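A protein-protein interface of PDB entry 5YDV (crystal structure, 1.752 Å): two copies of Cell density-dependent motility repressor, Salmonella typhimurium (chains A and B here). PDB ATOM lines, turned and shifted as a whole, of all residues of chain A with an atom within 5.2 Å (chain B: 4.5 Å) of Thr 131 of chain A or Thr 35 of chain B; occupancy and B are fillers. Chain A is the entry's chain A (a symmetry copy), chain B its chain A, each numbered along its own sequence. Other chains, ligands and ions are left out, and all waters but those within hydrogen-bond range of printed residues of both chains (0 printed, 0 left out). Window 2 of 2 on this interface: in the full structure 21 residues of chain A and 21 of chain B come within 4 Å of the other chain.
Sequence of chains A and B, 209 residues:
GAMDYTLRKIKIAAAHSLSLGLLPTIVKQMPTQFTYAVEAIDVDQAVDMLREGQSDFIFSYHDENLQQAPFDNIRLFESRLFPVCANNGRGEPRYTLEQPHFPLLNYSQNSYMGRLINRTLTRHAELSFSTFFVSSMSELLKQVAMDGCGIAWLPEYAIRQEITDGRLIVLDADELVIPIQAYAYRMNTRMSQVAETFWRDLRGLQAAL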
ATOM      1  N   LEU A 104     -21.550 -15.525  -1.502  1.00  0.00           N
ATOM      2  CA  LEU A 104     -22.277 -14.949  -2.619  1.00  0.00           C
ATOM      3  C   LEU A 104     -23.535 -15.765  -2.891  1.00  0.00           C
ATOM      4  O   LEU A 104     -23.494 -17.003  -2.901  1.00  0.00           O
ATOM      5  CB  LEU A 104     -21.393 -14.921  -3.873  1.00  0.00           C
ATOM      6  CG  LEU A 104     -22.057 -14.448  -5.167  1.00  0.00           C
ATOM      7  CD1 LEU A 104     -22.570 -13.021  -5.047  1.00  0.00           C
ATOM      8  CD2 LEU A 104     -21.142 -14.655  -6.386  1.00  0.00           C
ATOM      9  N   ASN A 106     -26.035 -16.087  -5.963  1.00  0.00           N
ATOM     10  CA  ASN A 106     -25.941 -15.682  -7.360  1.00  0.00           C
ATOM     11  C   ASN A 106     -26.970 -16.394  -8.234  1.00  0.00           C
ATOM     12  O   ASN A 106     -27.510 -17.442  -7.879  1.00  0.00           O
ATOM     13  CB  ASN A 106     -24.544 -15.949  -7.920  1.00  0.00           C
ATOM     14  CG  ASN A 106     -24.219 -15.055  -9.090  1.00  0.00           C
ATOM     15  OD1 ASN A 106     -24.978 -14.144  -9.415  1.00  0.00           O
ATOM     16  ND2 ASN A 106     -23.088 -15.300  -9.716  1.00  0.00           N
ATOM     17  N   PHE A 129     -14.959 -14.173  -3.259  1.00  0.00           N
ATOM     18  CA  PHE A 129     -16.240 -14.688  -2.805  1.00  0.00           C
ATOM     19  C   PHE A 129     -16.239 -16.202  -2.878  1.00  0.00           C
ATOM     20  O   PHE A 129     -15.478 -16.814  -3.634  1.00  0.00           O
ATOM     21  CB  PHE A 129     -17.408 -14.132  -3.642  1.00  0.00           C
ATOM     22  CG  PHE A 129     -17.269 -14.399  -5.112  1.00  0.00           C
ATOM     23  CD1 PHE A 129     -16.570 -13.520  -5.917  1.00  0.00           C
ATOM     24  CD2 PHE A 129     -17.795 -15.554  -5.677  1.00  0.00           C
ATOM     25  CE1 PHE A 129     -16.415 -13.771  -7.268  1.00  0.00           C
ATOM     26  CE2 PHE A 129     -17.649 -15.808  -7.025  1.00  0.00           C
ATOM     27  CZ  PHE A 129     -16.958 -14.913  -7.825  1.00  0.00           C
ATOM     28  N   SER A 130     -17.102 -16.805  -2.066  1.00  0.00           N
ATOM     29  CA  SER A 130     -17.457 -18.208  -2.194  1.00  0.00           C
ATOM     30  C   SER A 130     -18.947 -18.276  -2.488  1.00  0.00           C
ATOM     31  O   SER A 130     -19.743 -17.617  -1.818  1.00  0.00           O
ATOM     32  CB  SER A 130     -17.125 -18.996  -0.926  1.00  0.00           C
ATOM     33  OG  SER A 130     -17.945 -18.569   0.149  1.00  0.00           O
ATOM     34  N   THR A 131     -19.331 -19.065  -3.478  1.00  0.00           N
ATOM     35  CA  THR A 131     -20.735 -19.101  -3.871  1.00  0.00           C
ATOM     36  C   THR A 131     -21.505 -20.055  -2.958  1.00  0.00           C
ATOM     37  O   THR A 131     -21.303 -21.274  -2.996  1.00  0.00           O
ATOM     38  CB  THR A 131     -20.852 -19.500  -5.331  1.00  0.00           C
ATOM     39  OG1 THR A 131     -20.240 -18.477  -6.131  1.00  0.00           O
ATOM     40  CG2 THR A 131     -22.295 -19.590  -5.699  1.00  0.00           C
ATOM     41  N   PHE A 132     -22.390 -19.491  -2.135  1.00  0.00           N
ATOM     42  CA  PHE A 132     -23.162 -20.265  -1.172  1.00  0.00           C
ATOM     43  C   PHE A 132     -24.427 -20.862  -1.781  1.00  0.00           C
ATOM     44  O   PHE A 132     -24.816 -21.983  -1.436  1.00  0.00           O
ATOM     45  CB  PHE A 132     -23.519 -19.379   0.021  1.00  0.00           C
ATOM     46  CG  PHE A 132     -24.406 -20.046   1.032  1.00  0.00           C
ATOM     47  CD1 PHE A 132     -25.700 -19.588   1.239  1.00  0.00           C
ATOM     48  CD2 PHE A 132     -23.958 -21.138   1.761  1.00  0.00           C
ATOM     49  CE1 PHE A 132     -26.527 -20.207   2.169  1.00  0.00           C
ATOM     50  CE2 PHE A 132     -24.785 -21.752   2.690  1.00  0.00           C
ATOM     51  CZ  PHE A 132     -26.065 -21.282   2.891  1.00  0.00           C
ATOM     52  N   PHE A 133     -25.081 -20.134  -2.682  1.00  0.00           N
ATOM     53  CA  PHE A 133     -26.431 -20.473  -3.119  1.00  0.00           C
ATOM     54  C   PHE A 133     -26.589 -19.964  -4.541  1.00  0.00           C
ATOM     55  O   PHE A 133     -26.371 -18.773  -4.769  1.00  0.00           O
ATOM     56  CB  PHE A 133     -27.483 -19.817  -2.196  1.00  0.00           C
ATOM     57  CG  PHE A 133     -28.889 -20.303  -2.416  1.00  0.00           C
ATOM     58  CD1 PHE A 133     -29.409 -21.316  -1.625  1.00  0.00           C
ATOM     59  CD2 PHE A 133     -29.692 -19.746  -3.395  1.00  0.00           C
ATOM     60  CE1 PHE A 133     -30.698 -21.781  -1.823  1.00  0.00           C
ATOM     61  CE2 PHE A 133     -30.988 -20.205  -3.600  1.00  0.00           C
ATOM     62  CZ  PHE A 133     -31.491 -21.223  -2.804  1.00  0.00           C
ATOM     63  N   VAL A 134     -26.967 -20.843  -5.475  1.00  0.00           N
ATOM     64  CA  VAL A 134     -27.200 -20.484  -6.877  1.00  0.00           C
ATOM     65  C   VAL A 134     -28.620 -20.881  -7.246  1.00  0.00           C
ATOM     66  O   VAL A 134     -29.039 -22.011  -6.977  1.00  0.00           O
ATOM     67  CB  VAL A 134     -26.210 -21.170  -7.836  1.00  0.00           C
ATOM     68  CG1 VAL A 134     -26.488 -20.734  -9.291  1.00  0.00           C
ATOM     69  CG2 VAL A 134     -24.803 -20.828  -7.475  1.00  0.00           C
ATOM     70  N   THR B   6     -18.015 -30.081  -6.083  1.00  0.00           N
ATOM     71  CA  THR B   6     -17.256 -29.542  -4.964  1.00  0.00           C
ATOM     72  C   THR B   6     -17.494 -30.442  -3.758  1.00  0.00           C
ATOM     73  O   THR B   6     -18.362 -31.318  -3.774  1.00  0.00           O
ATOM     74  CB  THR B   6     -17.620 -28.089  -4.618  1.00  0.00           C
ATOM     75  OG1 THR B   6     -18.874 -28.059  -3.924  1.00  0.00           O
ATOM     76  CG2 THR B   6     -17.679 -27.184  -5.859  1.00  0.00           C
ATOM     77  N   ARG B   8     -18.761 -29.645  -0.995  1.00  0.00           N
ATOM     78  CA  ARG B   8     -19.927 -29.272  -0.202  1.00  0.00           C
ATOM     79  C   ARG B   8     -21.191 -29.034  -1.011  1.00  0.00           C
ATOM     80  O   ARG B   8     -22.246 -28.786  -0.410  1.00  0.00           O
ATOM     81  CB  ARG B   8     -19.633 -28.005   0.621  1.00  0.00           C
ATOM     82  CG  ARG B   8     -18.509 -28.157   1.630  1.00  0.00           C
ATOM     83  CD  ARG B   8     -18.197 -26.840   2.320  1.00  0.00           C
ATOM     84  NE  ARG B   8     -17.776 -25.813   1.374  1.00  0.00           N
ATOM     85  CZ  ARG B   8     -17.826 -24.507   1.615  1.00  0.00           C
ATOM     86  NH1 ARG B   8     -18.279 -24.059   2.779  1.00  0.00           N
ATOM     87  NH2 ARG B   8     -17.423 -23.643   0.691  1.00  0.00           N
ATOM     88  N   LYS B   9     -21.139 -29.105  -2.338  1.00  0.00           N
ATOM     89  CA  LYS B   9     -22.277 -28.666  -3.135  1.00  0.00           C
ATOM     90  C   LYS B   9     -23.375 -29.721  -3.090  1.00  0.00           C
ATOM     91  O   LYS B   9     -23.119 -30.919  -3.263  1.00  0.00           O
ATOM     92  CB  LYS B   9     -21.856 -28.376  -4.582  1.00  0.00           C
ATOM     93  CG  LYS B   9     -23.027 -28.209  -5.545  1.00  0.00           C
ATOM     94  CD  LYS B   9     -22.605 -27.689  -6.935  1.00  0.00           C
ATOM     95  CE  LYS B   9     -21.411 -26.756  -6.861  1.00  0.00           C
ATOM     96  NZ  LYS B   9     -21.406 -25.710  -7.940  1.00  0.00           N
ATOM     97  N   ILE B  10     -24.590 -29.272  -2.807  1.00  0.00           N
ATOM     98  CA  ILE B  10     -25.788 -30.093  -2.855  1.00  0.00           C
ATOM     99  C   ILE B  10     -26.627 -29.610  -4.028  1.00  0.00           C
ATOM    100  O   ILE B  10     -27.056 -28.449  -4.055  1.00  0.00           O
ATOM    101  CB  ILE B  10     -26.571 -30.003  -1.534  1.00  0.00           C
ATOM    102  CG1 ILE B  10     -25.709 -30.494  -0.363  1.00  0.00           C
ATOM    103  CG2 ILE B  10     -27.869 -30.797  -1.626  1.00  0.00           C
ATOM    104  CD1 ILE B  10     -25.447 -32.001  -0.381  1.00  0.00           C
ATOM    105  N   PHE B  34     -22.982 -26.877   3.934  1.00  0.00           N
ATOM    106  CA  PHE B  34     -23.360 -27.133   2.550  1.00  0.00           C
ATOM    107  C   PHE B  34     -23.348 -25.859   1.718  1.00  0.00           C
ATOM    108  O   PHE B  34     -23.466 -24.742   2.232  1.00  0.00           O
ATOM    109  CB  PHE B  34     -24.758 -27.757   2.442  1.00  0.00           C
ATOM    110  CG  PHE B  34     -24.983 -28.914   3.372  1.00  0.00           C
ATOM    111  CD1 PHE B  34     -24.380 -30.134   3.129  1.00  0.00           C
ATOM    112  CD2 PHE B  34     -25.817 -28.782   4.475  1.00  0.00           C
ATOM    113  CE1 PHE B  34     -24.583 -31.207   3.985  1.00  0.00           C
ATOM    114  CE2 PHE B  34     -26.029 -29.847   5.329  1.00  0.00           C
ATOM    115  CZ  PHE B  34     -25.415 -31.064   5.074  1.00  0.00           C
ATOM    116  N   THR B  35     -23.199 -26.049   0.415  1.00  0.00           N
ATOM    117  CA  THR B  35     -23.560 -25.025  -0.555  1.00  0.00           C
ATOM    118  C   THR B  35     -24.634 -25.600  -1.464  1.00  0.00           C
ATOM    119  O   THR B  35     -24.811 -26.821  -1.552  1.00  0.00           O
ATOM    120  CB  THR B  35     -22.367 -24.530  -1.374  1.00  0.00           C
ATOM    121  OG1 THR B  35     -21.852 -25.595  -2.178  1.00  0.00           O
ATOM    122  CG2 THR B  35     -21.280 -23.987  -0.460  1.00  0.00           C
ATOM    123  N   TYR B  36     -25.380 -24.712  -2.111  1.00  0.00           N
ATOM    124  CA  TYR B  36     -26.606 -25.114  -2.778  1.00  0.00           C
ATOM    125  C   TYR B  36     -26.612 -24.688  -4.233  1.00  0.00           C
ATOM    126  O   TYR B  36     -26.260 -23.550  -4.564  1.00  0.00           O
ATOM    127  CB  TYR B  36     -27.840 -24.531  -2.102  1.00  0.00           C
ATOM    128  CG  TYR B  36     -27.995 -24.950  -0.658  1.00  0.00           C
ATOM    129  CD1 TYR B  36     -27.307 -24.300   0.354  1.00  0.00           C
ATOM    130  CD2 TYR B  36     -28.810 -26.020  -0.321  1.00  0.00           C
ATOM    131  CE1 TYR B  36     -27.455 -24.684   1.687  1.00  0.00           C
ATOM    132  CE2 TYR B  36     -28.948 -26.427   0.999  1.00  0.00           C
ATOM    133  CZ  TYR B  36     -28.278 -25.752   1.996  1.00  0.00           C
ATOM    134  OH  TYR B  36     -28.421 -26.167   3.301  1.00  0.00           O
ATOM    135  N   ALA B  37     -27.060 -25.600  -5.092  1.00  0.00           N
ATOM    136  CA  ALA B  37     -27.394 -25.269  -6.470  1.00  0.00           C
ATOM    137  C   ALA B  37     -28.813 -25.751  -6.702  1.00  0.00           C
ATOM    138  O   ALA B  37     -29.082 -26.951  -6.584  1.00  0.00           O
ATOM    139  CB  ALA B  37     -26.420 -25.924  -7.458  1.00  0.00           C
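The backbone NH (N) of Val 134 of chain A lies within hydrogen-bond range of the backbone carbonyl oxygen (O) of Tyr 36 of chain B (2.9 Å).
The backbone carbonyl oxygen of Phe 132 of chain A sits at hydrogen-bond distance from the backbone NH of Tyr 36 of chain B.
The backbone carbonyl oxygen (O) of Arg 8 of chain B sits at hydrogen-bond distance from the backbone NH (N) of Thr 35 of chain B (3.0 Å).
N of Phe 132 of chain A sits at hydrogen-bond distance from O of Leu 104 of chain A (2.8 Å).
N of Ile 10 of chain B is in hydrogen-bond range of O of Thr 35 of chain B, 2.8 Å away.
O of Ile 10 of chain B sits at hydrogen-bond distance from N of Ala 37 of chain B (3.0 Å).
The backbone NH (N) of Asn 106 of chain A is in hydrogen-bond range of the backbone carbonyl oxygen (O) of Phe 133 of chain A, 3.0 Å away.
Thr 131 of chain A touches Thr 35 of chain B (O to CG2, 3.7 Å).
Phe 132 of chain A touches Phe 34 of chain B.
O of Phe 132 of chain A touches CA of Thr 35 of chain B (3.4 Å).
Tyr 36 of chain B touches Phe 133 of chain A.
Ala 37 of chain B touches Val 134 of chain A.
Of chain B, only Thr 35 comes within 4 Å of Thr 131 of chain A.
Thr 35 of chain B touches just these residues of chain A: Thr 131 and Phe 132.
Of the printed residues of chain B, Val 134 of chain A touches Tyr 36 and Ala 37.
Printed residues of chain A within 4 Å of Phe 34 of chain B: Phe 132.
Of the printed residues of chain A, Ala 37 of chain B touches Val 134 (3.7 Å).
Asn 106 of chain A touches none of the printed residues of chain B.
Arg 8 of chain B touches none of the printed residues of chain A.
The nearest printed residue of chain B that does not touch Thr 131 of chain A is Tyr 36 of chain B (5.4 Å).
The nearest printed residue of chain B that does not touch Phe 132 of chain A is Ala 37 of chain B (5.6 Å).
Hydrophobic or aromatic side chains of chain A that line the printed part of chain B: Phe 132 and Phe 133.
Hydrophobic or aromatic side chains of chain B that line the printed part of chain A: Tyr 36.
Among the printed residues, 7 pairs touch across the chains.
No position is printed for both chains.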
